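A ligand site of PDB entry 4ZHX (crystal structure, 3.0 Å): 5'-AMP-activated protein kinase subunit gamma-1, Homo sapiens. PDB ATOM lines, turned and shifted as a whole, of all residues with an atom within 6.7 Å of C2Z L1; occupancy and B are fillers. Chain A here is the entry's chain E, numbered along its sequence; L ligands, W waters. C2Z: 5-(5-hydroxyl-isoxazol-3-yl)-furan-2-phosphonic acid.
OG of Ser 319 sits at hydrogen-bond distance from OAC of C2Z L1, at 2.6 Å. A ring nitrogen (NE2) of His 156 sits at hydrogen-bond distance from an oxygen (OAD) of C2Z L1. An oxygen (OAC) of C2Z L2 lies within salt-bridge range of the guanidinium group (NH1) of Arg 157, 3.97 Å away. A ring nitrogen (ND1) of His 303 lies within hydrogen-bond range of a nitrogen (NAH) of C2Z L1 (3.1 Å). NH2 of Arg 304 is in salt-bridge range of OAB of C2Z L1 (2.9 Å). An oxygen (OAA) of C2Z L1 sits at hydrogen-bond distance from the guanidinium group (NH2) of Arg 157, 3.0 Å away. OG of Ser 231 lies within hydrogen-bond range of OAB of C2Z L1, at 3.2 Å. A ring nitrogen (ND1) of His 156 is in hydrogen-bond range of an oxygen (OAB) of C2Z L2 (2.7 Å). The side-chain hydroxyl of Ser 321 is in hydrogen-bond range of an oxygen (OAC) of C2Z L1.
An oxygen (OAA) of C2Z L1 lies close to a nitrogen (NAH) of C2Z L2 (3.5 Å).
The side-chain hydroxyl of Ser 319 is in hydrogen-bond range of the side-chain carboxylate of Asp 322 (2.7 Å). A ring nitrogen (NE2) of His 303 lies within hydrogen-bond range of the guanidinium group (NH1) of Arg 75 (3.0 Å). O of His 303 sits at hydrogen-bond distance from N of Leu 320. OG of Ser 319 is in hydrogen-bond range of OG of Ser 321 (2.9 Å).
Leu 320 touches C2Z L1. Hydrophobic or aromatic side chains that line C2Z L1: His 156, His 303 and Leu 320. Eight residues have an atom within 4 Å of C2Z L1: His 156, Arg 157, Ser 231, His 303, Arg 304, Ser 319, Leu 320 and Ser 321. The nearest printed residue that does not touch C2Z L1 is Asp 322 (4.4 Å).
Water W1 lies within hydrogen-bond range of O of His 156, N of His 174 and NAH of C2Z L1.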
ATOM      1  N   ARG A  75      31.160 -18.119  39.650  1.00  0.00           N
ATOM      2  CA  ARG A  75      30.832 -17.029  38.724  1.00  0.00           C
ATOM      3  C   ARG A  75      29.405 -16.479  38.881  1.00  0.00           C
ATOM      4  O   ARG A  75      29.170 -15.304  38.549  1.00  0.00           O
ATOM      5  CB  ARG A  75      31.135 -17.424  37.274  1.00  0.00           C
ATOM      6  CG  ARG A  75      32.633 -17.588  36.996  1.00  0.00           C
ATOM      7  CD  ARG A  75      32.925 -18.705  36.007  1.00  0.00           C
ATOM      8  NE  ARG A  75      33.081 -18.189  34.647  1.00  0.00           N
ATOM      9  CZ  ARG A  75      34.246 -18.044  34.027  1.00  0.00           C
ATOM     10  NH1 ARG A  75      34.292 -17.575  32.789  1.00  0.00           N
ATOM     11  NH2 ARG A  75      35.377 -18.358  34.645  1.00  0.00           N
ATOM     12  N   LYS A 154      18.325 -16.380  25.877  1.00  0.00           N
ATOM     13  CA  LYS A 154      19.623 -15.709  25.696  1.00  0.00           C
ATOM     14  C   LYS A 154      20.448 -15.593  27.002  1.00  0.00           C
ATOM     15  O   LYS A 154      21.159 -14.619  27.212  1.00  0.00           O
ATOM     16  CB  LYS A 154      19.506 -14.386  24.919  1.00  0.00           C
ATOM     17  CG  LYS A 154      19.245 -14.581  23.431  1.00  0.00           C
ATOM     18  CD  LYS A 154      19.227 -13.261  22.671  1.00  0.00           C
ATOM     19  CE  LYS A 154      18.906 -13.471  21.219  1.00  0.00           C
ATOM     20  NZ  LYS A 154      18.879 -12.183  20.469  1.00  0.00           N
ATOM     21  N   ILE A 155      20.322 -16.618  27.862  1.00  0.00           N
ATOM     22  CA  ILE A 155      21.024 -16.728  29.147  1.00  0.00           C
ATOM     23  C   ILE A 155      22.180 -17.723  29.057  1.00  0.00           C
ATOM     24  O   ILE A 155      22.150 -18.629  28.221  1.00  0.00           O
ATOM     25  CB  ILE A 155      20.056 -17.034  30.339  1.00  0.00           C
ATOM     26  CG1 ILE A 155      19.167 -18.271  30.066  1.00  0.00           C
ATOM     27  CG2 ILE A 155      19.214 -15.794  30.694  1.00  0.00           C
ATOM     28  CD1 ILE A 155      18.856 -19.103  31.282  1.00  0.00           C
ATOM     29  N   HIS A 156      23.188 -17.562  29.928  1.00  0.00           N
ATOM     30  CA  HIS A 156      24.369 -18.438  29.947  1.00  0.00           C
ATOM     31  C   HIS A 156      24.379 -19.398  31.126  1.00  0.00           C
ATOM     32  O   HIS A 156      25.117 -20.389  31.095  1.00  0.00           O
ATOM     33  CB  HIS A 156      25.659 -17.612  29.881  1.00  0.00           C
ATOM     34  CG  HIS A 156      25.694 -16.647  28.737  1.00  0.00           C
ATOM     35  ND1 HIS A 156      25.737 -15.280  28.945  1.00  0.00           N
ATOM     36  CD2 HIS A 156      25.631 -16.881  27.408  1.00  0.00           C
ATOM     37  CE1 HIS A 156      25.724 -14.732  27.743  1.00  0.00           C
ATOM     38  NE2 HIS A 156      25.671 -15.654  26.786  1.00  0.00           N
ATOM     39  N   ARG A 157      23.553 -19.124  32.152  1.00  0.00           N
ATOM     40  CA  ARG A 157      23.464 -19.960  33.351  1.00  0.00           C
ATOM     41  C   ARG A 157      22.028 -20.292  33.726  1.00  0.00           C
ATOM     42  O   ARG A 157      21.195 -19.396  33.880  1.00  0.00           O
ATOM     43  CB  ARG A 157      24.256 -19.354  34.514  1.00  0.00           C
ATOM     44  CG  ARG A 157      25.743 -19.602  34.349  1.00  0.00           C
ATOM     45  CD  ARG A 157      26.602 -18.973  35.412  1.00  0.00           C
ATOM     46  NE  ARG A 157      28.024 -19.119  35.086  1.00  0.00           N
ATOM     47  CZ  ARG A 157      28.729 -18.236  34.388  1.00  0.00           C
ATOM     48  NH1 ARG A 157      28.157 -17.120  33.944  1.00  0.00           N
ATOM     49  NH2 ARG A 157      30.006 -18.460  34.123  1.00  0.00           N
ATOM     50  N   THR A 173      25.556 -24.787  32.532  1.00  0.00           N
ATOM     51  CA  THR A 173      26.202 -23.872  31.569  1.00  0.00           C
ATOM     52  C   THR A 173      26.354 -24.528  30.194  1.00  0.00           C
ATOM     53  O   THR A 173      26.238 -25.752  30.085  1.00  0.00           O
ATOM     54  CB  THR A 173      27.592 -23.423  32.099  1.00  0.00           C
ATOM     55  OG1 THR A 173      28.423 -24.573  32.287  1.00  0.00           O
ATOM     56  CG2 THR A 173      27.512 -22.621  33.386  1.00  0.00           C
ATOM     57  N   HIS A 174      26.670 -23.717  29.157  1.00  0.00           N
ATOM     58  CA  HIS A 174      26.918 -24.173  27.780  1.00  0.00           C
ATOM     59  C   HIS A 174      28.185 -25.025  27.719  1.00  0.00           C
ATOM     60  O   HIS A 174      28.273 -25.953  26.914  1.00  0.00           O
ATOM     61  CB  HIS A 174      27.060 -22.972  26.841  1.00  0.00           C
ATOM     62  CG  HIS A 174      25.777 -22.259  26.540  1.00  0.00           C
ATOM     63  ND1 HIS A 174      25.410 -21.126  27.242  1.00  0.00           N
ATOM     64  CD2 HIS A 174      24.831 -22.526  25.614  1.00  0.00           C
ATOM     65  CE1 HIS A 174      24.246 -20.755  26.726  1.00  0.00           C
ATOM     66  NE2 HIS A 174      23.858 -21.562  25.743  1.00  0.00           N
ATOM     67  N   LYS A 175      29.172 -24.693  28.574  1.00  0.00           N
ATOM     68  CA  LYS A 175      30.472 -25.352  28.712  1.00  0.00           C
ATOM     69  C   LYS A 175      30.302 -26.792  29.233  1.00  0.00           C
ATOM     70  O   LYS A 175      30.987 -27.690  28.737  1.00  0.00           O
ATOM     71  CB  LYS A 175      31.373 -24.538  29.652  1.00  0.00           C
ATOM     72  CG  LYS A 175      32.832 -24.951  29.662  1.00  0.00           C
ATOM     73  CD  LYS A 175      33.622 -24.113  30.653  1.00  0.00           C
ATOM     74  CE  LYS A 175      34.990 -24.690  30.921  1.00  0.00           C
ATOM     75  NZ  LYS A 175      35.763 -23.837  31.868  1.00  0.00           N
ATOM     76  N   THR A 205      28.933 -15.330  14.788  1.00  0.00           N
ATOM     77  CA  THR A 205      28.735 -13.923  14.446  1.00  0.00           C
ATOM     78  C   THR A 205      29.916 -13.465  13.592  1.00  0.00           C
ATOM     79  O   THR A 205      31.066 -13.593  14.031  1.00  0.00           O
ATOM     80  CB  THR A 205      28.547 -13.077  15.721  1.00  0.00           C
ATOM     81  OG1 THR A 205      27.579 -13.708  16.572  1.00  0.00           O
ATOM     82  CG2 THR A 205      28.093 -11.645  15.425  1.00  0.00           C
ATOM     83  N   ARG A 229      25.064  -5.858  24.647  1.00  0.00           N
ATOM     84  CA  ARG A 229      24.694  -7.101  25.357  1.00  0.00           C
ATOM     85  C   ARG A 229      25.576  -8.311  25.010  1.00  0.00           C
ATOM     86  O   ARG A 229      25.118  -9.455  25.008  1.00  0.00           O
ATOM     87  CB  ARG A 229      23.183  -7.401  25.254  1.00  0.00           C
ATOM     88  CG  ARG A 229      22.341  -6.614  26.254  1.00  0.00           C
ATOM     89  CD  ARG A 229      20.874  -6.984  26.147  1.00  0.00           C
ATOM     90  NE  ARG A 229      20.097  -6.448  27.276  1.00  0.00           N
ATOM     91  CZ  ARG A 229      19.820  -7.126  28.380  1.00  0.00           C
ATOM     92  NH1 ARG A 229      20.251  -8.376  28.526  1.00  0.00           N
ATOM     93  NH2 ARG A 229      19.107  -6.571  29.343  1.00  0.00           N
ATOM     94  N   VAL A 230      26.875  -8.052  24.735  1.00  0.00           N
ATOM     95  CA  VAL A 230      27.888  -9.057  24.412  1.00  0.00           C
ATOM     96  C   VAL A 230      28.622  -9.542  25.677  1.00  0.00           C
ATOM     97  O   VAL A 230      28.595  -8.844  26.689  1.00  0.00           O
ATOM     98  CB  VAL A 230      28.868  -8.610  23.292  1.00  0.00           C
ATOM     99  CG1 VAL A 230      28.184  -8.591  21.923  1.00  0.00           C
ATOM    100  CG2 VAL A 230      29.517  -7.251  23.596  1.00  0.00           C
ATOM    101  N   SER A 231      29.254 -10.726  25.609  1.00  0.00           N
ATOM    102  CA  SER A 231      29.975 -11.313  26.753  1.00  0.00           C
ATOM    103  C   SER A 231      31.469 -11.011  26.794  1.00  0.00           C
ATOM    104  O   SER A 231      32.047 -10.978  27.882  1.00  0.00           O
ATOM    105  CB  SER A 231      29.724 -12.818  26.820  1.00  0.00           C
ATOM    106  OG  SER A 231      28.369 -13.097  27.118  1.00  0.00           O
ATOM    107  N   ALA A 232      32.111 -10.818  25.620  1.00  0.00           N
ATOM    108  CA  ALA A 232      33.540 -10.527  25.541  1.00  0.00           C
ATOM    109  C   ALA A 232      33.890  -9.516  24.453  1.00  0.00           C
ATOM    110  O   ALA A 232      33.193  -9.442  23.433  1.00  0.00           O
ATOM    111  CB  ALA A 232      34.337 -11.802  25.323  1.00  0.00           C
ATOM    112  N   HIS A 303      35.372 -20.083  26.341  1.00  0.00           N
ATOM    113  CA  HIS A 303      33.988 -19.907  25.888  1.00  0.00           C
ATOM    114  C   HIS A 303      33.862 -19.490  24.418  1.00  0.00           C
ATOM    115  O   HIS A 303      32.807 -19.713  23.824  1.00  0.00           O
ATOM    116  CB  HIS A 303      33.234 -18.929  26.800  1.00  0.00           C
ATOM    117  CG  HIS A 303      33.283 -19.273  28.255  1.00  0.00           C
ATOM    118  ND1 HIS A 303      32.572 -20.345  28.768  1.00  0.00           N
ATOM    119  CD2 HIS A 303      33.947 -18.666  29.266  1.00  0.00           C
ATOM    120  CE1 HIS A 303      32.840 -20.363  30.062  1.00  0.00           C
ATOM    121  NE2 HIS A 303      33.660 -19.371  30.410  1.00  0.00           N
ATOM    122  N   ARG A 304      34.942 -18.887  23.830  1.00  0.00           N
ATOM    123  CA  ARG A 304      34.939 -18.473  22.432  1.00  0.00           C
ATOM    124  C   ARG A 304      36.271 -18.648  21.714  1.00  0.00           C
ATOM    125  O   ARG A 304      37.316 -18.822  22.357  1.00  0.00           O
ATOM    126  CB  ARG A 304      34.351 -17.064  22.240  1.00  0.00           C
ATOM    127  CG  ARG A 304      35.075 -15.943  22.976  1.00  0.00           C
ATOM    128  CD  ARG A 304      34.213 -14.701  23.083  1.00  0.00           C
ATOM    129  NE  ARG A 304      33.141 -14.857  24.058  1.00  0.00           N
ATOM    130  CZ  ARG A 304      31.861 -15.049  23.756  1.00  0.00           C
ATOM    131  NH1 ARG A 304      31.468 -15.101  22.486  1.00  0.00           N
ATOM    132  NH2 ARG A 304      30.958 -15.191  24.722  1.00  0.00           N
ATOM    133  N   ILE A 317      33.558 -14.317  15.412  1.00  0.00           N
ATOM    134  CA  ILE A 317      33.707 -14.976  16.713  1.00  0.00           C
ATOM    135  C   ILE A 317      32.757 -16.168  16.795  1.00  0.00           C
ATOM    136  O   ILE A 317      31.551 -16.012  16.574  1.00  0.00           O
ATOM    137  CB  ILE A 317      33.491 -13.969  17.901  1.00  0.00           C
ATOM    138  CG1 ILE A 317      34.432 -12.722  17.841  1.00  0.00           C
ATOM    139  CG2 ILE A 317      33.524 -14.650  19.280  1.00  0.00           C
ATOM    140  CD1 ILE A 317      35.980 -12.935  18.008  1.00  0.00           C
ATOM    141  N   VAL A 318      33.293 -17.361  17.117  1.00  0.00           N
ATOM    142  CA  VAL A 318      32.507 -18.579  17.293  1.00  0.00           C
ATOM    143  C   VAL A 318      32.531 -19.010  18.769  1.00  0.00           C
ATOM    144  O   VAL A 318      33.603 -19.167  19.357  1.00  0.00           O
ATOM    145  CB  VAL A 318      32.827 -19.709  16.271  1.00  0.00           C
ATOM    146  CG1 VAL A 318      34.259 -20.240  16.411  1.00  0.00           C
ATOM    147  CG2 VAL A 318      31.810 -20.849  16.341  1.00  0.00           C
ATOM    148  N   SER A 319      31.340 -19.117  19.389  1.00  0.00           N
ATOM    149  CA  SER A 319      31.172 -19.466  20.801  1.00  0.00           C
ATOM    150  C   SER A 319      30.432 -20.786  21.012  1.00  0.00           C
ATOM    151  O   SER A 319      29.968 -21.400  20.051  1.00  0.00           O
ATOM    152  CB  SER A 319      30.456 -18.334  21.531  1.00  0.00           C
ATOM    153  OG  SER A 319      29.166 -18.102  20.987  1.00  0.00           O
ATOM    154  N   LEU A 320      30.328 -21.219  22.289  1.00  0.00           N
ATOM    155  CA  LEU A 320      29.636 -22.446  22.715  1.00  0.00           C
ATOM    156  C   LEU A 320      28.149 -22.380  22.374  1.00  0.00           C
ATOM    157  O   LEU A 320      27.563 -23.392  21.970  1.00  0.00           O
ATOM    158  CB  LEU A 320      29.813 -22.704  24.228  1.00  0.00           C
ATOM    159  CG  LEU A 320      31.218 -22.584  24.824  1.00  0.00           C
ATOM    160  CD1 LEU A 320      31.145 -22.429  26.329  1.00  0.00           C
ATOM    161  CD2 LEU A 320      32.082 -23.784  24.491  1.00  0.00           C
ATOM    162  N   SER A 321      27.541 -21.183  22.516  1.00  0.00           N
ATOM    163  CA  SER A 321      26.119 -20.920  22.230  1.00  0.00           C
ATOM    164  C   SER A 321      25.795 -21.100  20.739  1.00  0.00           C
ATOM    165  O   SER A 321      24.714 -21.598  20.424  1.00  0.00           O
ATOM    166  CB  SER A 321      25.729 -19.526  22.700  1.00  0.00           C
ATOM    167  OG  SER A 321      26.499 -18.519  22.064  1.00  0.00           O
ATOM    168  N   ASP A 322      26.722 -20.712  19.844  1.00  0.00           N
ATOM    169  CA  ASP A 322      26.578 -20.835  18.386  1.00  0.00           C
ATOM    170  C   ASP A 322      26.649 -22.305  17.953  1.00  0.00           C
ATOM    171  O   ASP A 322      25.860 -22.719  17.092  1.00  0.00           O
ATOM    172  CB  ASP A 322      27.638 -20.000  17.651  1.00  0.00           C
ATOM    173  CG  ASP A 322      27.498 -18.495  17.838  1.00  0.00           C
ATOM    174  OD1 ASP A 322      26.485 -17.938  17.377  1.00  0.00           O
ATOM    175  OD2 ASP A 322      28.439 -17.885  18.382  1.00  0.00           O
HETATM  176  OAB C2Z L   1      28.235 -14.440  24.259  1.00  0.00           O
HETATM  177  PAO C2Z L   1      27.673 -15.918  23.936  1.00  0.00           P
HETATM  178  OAD C2Z L   1      26.072 -15.795  24.015  1.00  0.00           O
HETATM  179  OAA C2Z L   1      29.641 -17.441  31.372  1.00  0.00           O
HETATM  180  CAN C2Z L   1      28.308 -17.155  25.030  1.00  0.00           C
HETATM  181  OAJ C2Z L   1      28.483 -16.984  26.341  1.00  0.00           O
HETATM  182  CAF C2Z L   1      28.678 -18.390  24.677  1.00  0.00           C
HETATM  183  CAE C2Z L   1      29.096 -19.013  25.783  1.00  0.00           C
HETATM  184  CAM C2Z L   1      28.979 -18.152  26.793  1.00  0.00           C
HETATM  185  CAL C2Z L   1      29.268 -18.396  28.071  1.00  0.00           C
HETATM  186  CAG C2Z L   1      29.236 -17.485  29.037  1.00  0.00           C
HETATM  187  NAH C2Z L   1      29.574 -19.593  28.579  1.00  0.00           N
HETATM  188  OAI C2Z L   1      29.769 -19.396  29.965  1.00  0.00           O
HETATM  189  CAK C2Z L   1      29.555 -18.081  30.180  1.00  0.00           C
HETATM  190  OAC C2Z L   1      28.014 -16.174  22.390  1.00  0.00           O
HETATM  191  OAB C2Z L   2      25.018 -13.298  30.669  1.00  0.00           O
HETATM  192  PAO C2Z L   2      25.632 -13.699  32.100  1.00  0.00           P
HETATM  193  OAD C2Z L   2      24.940 -12.705  33.145  1.00  0.00           O
HETATM  194  OAA C2Z L   2      33.917 -14.814  30.485  1.00  0.00           O
HETATM  195  CAN C2Z L   2      27.397 -13.646  32.133  1.00  0.00           C
HETATM  196  OAJ C2Z L   2      28.193 -14.135  31.174  1.00  0.00           O
HETATM  197  CAF C2Z L   2      28.124 -13.110  33.114  1.00  0.00           C
HETATM  198  CAE C2Z L   2      29.408 -13.263  32.788  1.00  0.00           C
HETATM  199  CAM C2Z L   2      29.450 -13.886  31.604  1.00  0.00           C
HETATM  200  CAL C2Z L   2      30.546 -14.219  30.913  1.00  0.00           C
HETATM  201  CAG C2Z L   2      31.790 -14.281  31.384  1.00  0.00           C
HETATM  202  NAH C2Z L   2      30.523 -14.557  29.625  1.00  0.00           N
HETATM  203  OAI C2Z L   2      31.834 -14.838  29.259  1.00  0.00           O
HETATM  204  CAK C2Z L   2      32.577 -14.658  30.375  1.00  0.00           C
HETATM  205  OAC C2Z L   2      25.048 -15.172  32.434  1.00  0.00           O
HETATM  206  O   HOH W   1      27.312 -20.992  29.646  1.00  0.00           O
